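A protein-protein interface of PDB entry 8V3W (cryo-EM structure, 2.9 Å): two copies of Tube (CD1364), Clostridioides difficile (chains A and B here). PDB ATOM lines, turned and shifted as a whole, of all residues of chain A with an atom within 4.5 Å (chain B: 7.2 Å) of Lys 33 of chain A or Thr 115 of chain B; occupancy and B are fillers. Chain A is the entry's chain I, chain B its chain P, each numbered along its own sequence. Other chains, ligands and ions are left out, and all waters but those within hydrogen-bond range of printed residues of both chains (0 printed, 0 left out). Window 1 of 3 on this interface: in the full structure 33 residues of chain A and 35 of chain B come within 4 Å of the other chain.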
ATOM      1  N   ALA A  32      25.753  23.812  -7.876  1.00  0.00           N
ATOM      2  CA  ALA A  32      26.849  24.635  -8.371  1.00  0.00           C
ATOM      3  C   ALA A  32      26.388  25.327  -9.643  1.00  0.00           C
ATOM      4  O   ALA A  32      25.864  24.670 -10.543  1.00  0.00           O
ATOM      5  CB  ALA A  32      28.097  23.792  -8.631  1.00  0.00           C
ATOM      6  N   LYS A  33      26.579  26.642  -9.717  1.00  0.00           N
ATOM      7  CA  LYS A  33      26.015  27.419 -10.813  1.00  0.00           C
ATOM      8  C   LYS A  33      26.860  28.655 -11.078  1.00  0.00           C
ATOM      9  O   LYS A  33      27.340  29.297 -10.143  1.00  0.00           O
ATOM     10  CB  LYS A  33      24.572  27.818 -10.498  1.00  0.00           C
ATOM     11  CG  LYS A  33      23.894  28.628 -11.570  1.00  0.00           C
ATOM     12  CD  LYS A  33      22.720  29.392 -11.009  1.00  0.00           C
ATOM     13  CE  LYS A  33      21.601  28.453 -10.604  1.00  0.00           C
ATOM     14  NZ  LYS A  33      20.390  29.193 -10.167  1.00  0.00           N
ATOM     15  N   MET A  34      27.028  28.987 -12.354  1.00  0.00           N
ATOM     16  CA  MET A  34      27.745  30.181 -12.783  1.00  0.00           C
ATOM     17  C   MET A  34      26.747  31.273 -13.149  1.00  0.00           C
ATOM     18  O   MET A  34      25.799  31.021 -13.893  1.00  0.00           O
ATOM     19  CB  MET A  34      28.637  29.876 -13.985  1.00  0.00           C
ATOM     20  CG  MET A  34      30.038  29.441 -13.635  1.00  0.00           C
ATOM     21  SD  MET A  34      31.077  30.809 -13.113  1.00  0.00           S
ATOM     22  CE  MET A  34      32.294  29.943 -12.137  1.00  0.00           C
ATOM     23  N   GLU A  35      26.964  32.479 -12.634  1.00  0.00           N
ATOM     24  CA  GLU A  35      26.106  33.623 -12.912  1.00  0.00           C
ATOM     25  C   GLU A  35      26.841  34.652 -13.757  1.00  0.00           C
ATOM     26  O   GLU A  35      27.994  34.980 -13.480  1.00  0.00           O
ATOM     27  CB  GLU A  35      25.628  34.285 -11.623  1.00  0.00           C
ATOM     28  CG  GLU A  35      24.301  33.782 -11.132  1.00  0.00           C
ATOM     29  CD  GLU A  35      24.443  32.849  -9.962  1.00  0.00           C
ATOM     30  OE1 GLU A  35      25.525  32.842  -9.342  1.00  0.00           O
ATOM     31  OE2 GLU A  35      23.475  32.123  -9.663  1.00  0.00           O
ATOM     32  N   LYS A  57      30.468  34.897 -11.920  1.00  0.00           N
ATOM     33  CA  LYS A  57      30.713  34.478 -10.548  1.00  0.00           C
ATOM     34  C   LYS A  57      30.110  33.095 -10.339  1.00  0.00           C
ATOM     35  O   LYS A  57      29.185  32.701 -11.049  1.00  0.00           O
ATOM     36  CB  LYS A  57      30.117  35.476  -9.555  1.00  0.00           C
ATOM     37  CG  LYS A  57      30.710  35.402  -8.170  1.00  0.00           C
ATOM     38  CD  LYS A  57      29.971  36.303  -7.206  1.00  0.00           C
ATOM     39  CE  LYS A  57      30.814  36.590  -5.981  1.00  0.00           C
ATOM     40  NZ  LYS A  57      31.007  35.365  -5.172  1.00  0.00           N
ATOM     41  N   GLY A  58      30.634  32.364  -9.366  1.00  0.00           N
ATOM     42  CA  GLY A  58      30.172  31.013  -9.069  1.00  0.00           C
ATOM     43  C   GLY A  58      29.564  30.909  -7.683  1.00  0.00           C
ATOM     44  O   GLY A  58      30.065  31.512  -6.736  1.00  0.00           O
ATOM     45  N   LYS A  59      28.479  30.141  -7.574  1.00  0.00           N
ATOM     46  CA  LYS A  59      27.768  29.950  -6.316  1.00  0.00           C
ATOM     47  C   LYS A  59      27.240  28.524  -6.233  1.00  0.00           C
ATOM     48  O   LYS A  59      26.976  27.881  -7.249  1.00  0.00           O
ATOM     49  CB  LYS A  59      26.604  30.935  -6.170  1.00  0.00           C
ATOM     50  CG  LYS A  59      27.017  32.390  -6.110  1.00  0.00           C
ATOM     51  CD  LYS A  59      26.000  33.251  -5.378  1.00  0.00           C
ATOM     52  CE  LYS A  59      24.620  32.614  -5.353  1.00  0.00           C
ATOM     53  NZ  LYS A  59      23.579  33.594  -4.938  1.00  0.00           N
ATOM     54  N   PHE A 133      32.832  29.872  -5.635  1.00  0.00           N
ATOM     55  CA  PHE A 133      33.984  29.294  -6.313  1.00  0.00           C
ATOM     56  C   PHE A 133      34.297  30.127  -7.549  1.00  0.00           C
ATOM     57  O   PHE A 133      33.568  31.061  -7.889  1.00  0.00           O
ATOM     58  CB  PHE A 133      33.737  27.825  -6.669  1.00  0.00           C
ATOM     59  CG  PHE A 133      32.640  27.611  -7.672  1.00  0.00           C
ATOM     60  CD1 PHE A 133      31.316  27.640  -7.288  1.00  0.00           C
ATOM     61  CD2 PHE A 133      32.937  27.363  -8.997  1.00  0.00           C
ATOM     62  CE1 PHE A 133      30.315  27.437  -8.208  1.00  0.00           C
ATOM     63  CE2 PHE A 133      31.939  27.161  -9.917  1.00  0.00           C
ATOM     64  CZ  PHE A 133      30.628  27.196  -9.522  1.00  0.00           C
ATOM     65  N   HIS B  66      16.523  16.931 -17.261  1.00  0.00           N
ATOM     66  CA  HIS B  66      17.966  16.712 -17.266  1.00  0.00           C
ATOM     67  C   HIS B  66      18.254  15.311 -17.792  1.00  0.00           C
ATOM     68  O   HIS B  66      18.197  14.331 -17.049  1.00  0.00           O
ATOM     69  CB  HIS B  66      18.550  16.917 -15.875  1.00  0.00           C
ATOM     70  CG  HIS B  66      20.044  16.895 -15.845  1.00  0.00           C
ATOM     71  ND1 HIS B  66      20.816  17.465 -16.831  1.00  0.00           N
ATOM     72  CD2 HIS B  66      20.909  16.369 -14.948  1.00  0.00           C
ATOM     73  CE1 HIS B  66      22.093  17.294 -16.543  1.00  0.00           C
ATOM     74  NE2 HIS B  66      22.177  16.630 -15.406  1.00  0.00           N
ATOM     75  N   MET B  71      23.343  22.363 -22.359  1.00  0.00           N
ATOM     76  CA  MET B  71      23.675  23.775 -22.191  1.00  0.00           C
ATOM     77  C   MET B  71      25.178  23.998 -22.115  1.00  0.00           C
ATOM     78  O   MET B  71      25.682  25.005 -22.622  1.00  0.00           O
ATOM     79  CB  MET B  71      22.989  24.336 -20.949  1.00  0.00           C
ATOM     80  CG  MET B  71      21.480  24.332 -21.022  1.00  0.00           C
ATOM     81  SD  MET B  71      20.862  25.863 -21.737  1.00  0.00           S
ATOM     82  CE  MET B  71      20.249  25.255 -23.295  1.00  0.00           C
ATOM     83  N   HIS B  72      25.910  23.093 -21.465  1.00  0.00           N
ATOM     84  CA  HIS B  72      27.355  23.269 -21.375  1.00  0.00           C
ATOM     85  C   HIS B  72      28.014  23.164 -22.743  1.00  0.00           C
ATOM     86  O   HIS B  72      28.906  23.954 -23.070  1.00  0.00           O
ATOM     87  CB  HIS B  72      27.965  22.249 -20.421  1.00  0.00           C
ATOM     88  CG  HIS B  72      29.450  22.135 -20.548  1.00  0.00           C
ATOM     89  ND1 HIS B  72      30.067  21.059 -21.146  1.00  0.00           N
ATOM     90  CD2 HIS B  72      30.442  22.977 -20.175  1.00  0.00           C
ATOM     91  CE1 HIS B  72      31.375  21.236 -21.124  1.00  0.00           C
ATOM     92  NE2 HIS B  72      31.629  22.394 -20.542  1.00  0.00           N
ATOM     93  N   ASP B 113      22.586  32.470 -17.045  1.00  0.00           N
ATOM     94  CA  ASP B 113      23.445  31.700 -16.155  1.00  0.00           C
ATOM     95  C   ASP B 113      23.649  30.314 -16.753  1.00  0.00           C
ATOM     96  O   ASP B 113      23.098  29.985 -17.806  1.00  0.00           O
ATOM     97  CB  ASP B 113      22.861  31.625 -14.740  1.00  0.00           C
ATOM     98  CG  ASP B 113      21.475  31.016 -14.703  1.00  0.00           C
ATOM     99  OD1 ASP B 113      21.338  29.807 -14.978  1.00  0.00           O
ATOM    100  OD2 ASP B 113      20.517  31.749 -14.389  1.00  0.00           O
ATOM    101  N   LEU B 114      24.463  29.507 -16.077  1.00  0.00           N
ATOM    102  CA  LEU B 114      24.718  28.130 -16.474  1.00  0.00           C
ATOM    103  C   LEU B 114      24.724  27.248 -15.236  1.00  0.00           C
ATOM    104  O   LEU B 114      25.449  27.527 -14.280  1.00  0.00           O
ATOM    105  CB  LEU B 114      26.050  28.003 -17.220  1.00  0.00           C
ATOM    106  CG  LEU B 114      26.519  26.586 -17.544  1.00  0.00           C
ATOM    107  CD1 LEU B 114      25.647  25.965 -18.608  1.00  0.00           C
ATOM    108  CD2 LEU B 114      27.966  26.599 -17.989  1.00  0.00           C
ATOM    109  N   THR B 115      23.926  26.186 -15.256  1.00  0.00           N
ATOM    110  CA  THR B 115      23.837  25.256 -14.140  1.00  0.00           C
ATOM    111  C   THR B 115      24.760  24.076 -14.409  1.00  0.00           C
ATOM    112  O   THR B 115      24.649  23.420 -15.447  1.00  0.00           O
ATOM    113  CB  THR B 115      22.403  24.772 -13.936  1.00  0.00           C
ATOM    114  OG1 THR B 115      21.610  25.839 -13.410  1.00  0.00           O
ATOM    115  CG2 THR B 115      22.371  23.615 -12.959  1.00  0.00           C
ATOM    116  N   LEU B 116      25.672  23.816 -13.476  1.00  0.00           N
ATOM    117  CA  LEU B 116      26.621  22.721 -13.612  1.00  0.00           C
ATOM    118  C   LEU B 116      26.121  21.451 -12.939  1.00  0.00           C
ATOM    119  O   LEU B 116      26.203  20.365 -13.518  1.00  0.00           O
ATOM    120  CB  LEU B 116      27.977  23.128 -13.033  1.00  0.00           C
ATOM    121  CG  LEU B 116      28.529  24.470 -13.506  1.00  0.00           C
ATOM    122  CD1 LEU B 116      29.793  24.811 -12.758  1.00  0.00           C
ATOM    123  CD2 LEU B 116      28.788  24.434 -14.991  1.00  0.00           C
ATOM    124  N   ALA B 117      25.603  21.567 -11.723  1.00  0.00           N
ATOM    125  CA  ALA B 117      25.082  20.417 -11.001  1.00  0.00           C
ATOM    126  C   ALA B 117      23.996  20.888 -10.051  1.00  0.00           C
ATOM    127  O   ALA B 117      24.175  21.888  -9.353  1.00  0.00           O
ATOM    128  CB  ALA B 117      26.189  19.698 -10.229  1.00  0.00           C
ATOM    129  N   ASP B 118      22.866  20.188 -10.053  1.00  0.00           N
ATOM    130  CA  ASP B 118      21.792  20.462  -9.099  1.00  0.00           C
ATOM    131  C   ASP B 118      20.994  19.169  -8.932  1.00  0.00           C
ATOM    132  O   ASP B 118      20.056  18.907  -9.687  1.00  0.00           O
ATOM    133  CB  ASP B 118      20.922  21.618  -9.574  1.00  0.00           C
ATOM    134  CG  ASP B 118      19.700  21.828  -8.706  1.00  0.00           C
ATOM    135  OD1 ASP B 118      19.818  21.742  -7.467  1.00  0.00           O
ATOM    136  OD2 ASP B 118      18.615  22.088  -9.265  1.00  0.00           O
ATOM    137  N   GLU B 126      15.929  18.661 -13.196  1.00  0.00           N
ATOM    138  CA  GLU B 126      15.439  19.635 -14.160  1.00  0.00           C
ATOM    139  C   GLU B 126      16.404  20.809 -14.237  1.00  0.00           C
ATOM    140  O   GLU B 126      17.160  21.081 -13.303  1.00  0.00           O
ATOM    141  CB  GLU B 126      14.040  20.143 -13.801  1.00  0.00           C
ATOM    142  CG  GLU B 126      12.949  19.107 -13.930  1.00  0.00           C
ATOM    143  CD  GLU B 126      11.633  19.585 -13.370  1.00  0.00           C
ATOM    144  OE1 GLU B 126      11.564  20.745 -12.911  1.00  0.00           O
ATOM    145  OE2 GLU B 126      10.659  18.804 -13.395  1.00  0.00           O
ATOM    146  N   ILE B 127      16.357  21.514 -15.364  1.00  0.00           N
ATOM    147  CA  ILE B 127      17.221  22.654 -15.638  1.00  0.00           C
ATOM    148  C   ILE B 127      16.348  23.846 -16.004  1.00  0.00           C
ATOM    149  O   ILE B 127      15.370  23.701 -16.745  1.00  0.00           O
ATOM    150  CB  ILE B 127      18.216  22.351 -16.778  1.00  0.00           C
ATOM    151  CG1 ILE B 127      19.008  21.079 -16.484  1.00  0.00           C
ATOM    152  CG2 ILE B 127      19.150  23.522 -16.998  1.00  0.00           C
ATOM    153  CD1 ILE B 127      19.825  21.147 -15.225  1.00  0.00           C
ATOM    154  N   GLU B 128      16.698  25.022 -15.491  1.00  0.00           N
ATOM    155  CA  GLU B 128      16.006  26.264 -15.807  1.00  0.00           C
ATOM    156  C   GLU B 128      16.998  27.273 -16.367  1.00  0.00           C
ATOM    157  O   GLU B 128      18.076  27.466 -15.797  1.00  0.00           O
ATOM    158  CB  GLU B 128      15.318  26.830 -14.569  1.00  0.00           C
ATOM    159  CG  GLU B 128      14.523  28.080 -14.830  1.00  0.00           C
ATOM    160  CD  GLU B 128      13.242  28.111 -14.040  1.00  0.00           C
ATOM    161  OE1 GLU B 128      13.060  27.225 -13.181  1.00  0.00           O
ATOM    162  OE2 GLU B 128      12.420  29.023 -14.270  1.00  0.00           O
ATOM    163  N   ALA B 129      16.629  27.930 -17.466  1.00  0.00           N
ATOM    164  CA  ALA B 129      17.549  28.798 -18.199  1.00  0.00           C
ATOM    165  C   ALA B 129      16.861  30.075 -18.669  1.00  0.00           C
ATOM    166  O   ALA B 129      16.263  30.101 -19.756  1.00  0.00           O
ATOM    167  CB  ALA B 129      18.155  28.046 -19.380  1.00  0.00           C
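O of Ala 32 of chain A lies within hydrogen-bond range of N of Leu 116 of chain B, at 3.1 Å.
The backbone NH of Ala 32 of chain A lies within hydrogen-bond range of the backbone carbonyl oxygen of Ala 117 of chain B, 2.9 Å away.
The backbone NH (N) of Met 34 of chain A sits at hydrogen-bond distance from the backbone carbonyl oxygen (O) of Leu 114 of chain B.
The backbone NH (N) of Lys 33 of chain A lies within hydrogen-bond range of the backbone carbonyl oxygen (O) of Lys 59 of chain A, at 2.8 Å.
O of Leu 114 of chain B touches CG of Lys 33 of chain A, at 3.3 Å.
CE of Lys 33 of chain A touches OG1 of Thr 115 of chain B, 3.8 Å away.
O of Met 34 of chain A touches CB of Asp 113 of chain B, at 3.1 Å.
Lys 33 of chain A touches two residues of chain B.
Thr 115 of chain B touches one residue of chain A.
Of the printed residues of chain A, Leu 116 of chain B touches Ala 32.
Of the printed residues of chain B, Ala 32 of chain A touches Leu 116 and Ala 117.
Printed residues of chain B within 4 Å of Met 34 of chain A: Asp 113 and Leu 114.
Of the printed residues of chain A, Asp 113 of chain B touches Met 34 (3.1 Å).
The nearest printed residue of chain A that does not touch Ala 117 of chain B is Lys 33 of chain A (5.3 Å).
Of the 8 printed residues of chain A, 3 touch a printed residue of chain B.
Printed residues of chain A that touch a printed residue of chain B: Ala 32, Lys 33 and Met 34.
Among the printed residues, no Asp or Glu carboxylate lies within 4 Å of a Lys or Arg side-chain nitrogen of the other chain.
No position is printed for both chains.
Of the 6 pairs that touch across the chains among the printed residues, none has its exchanged pair printed and touching as well.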
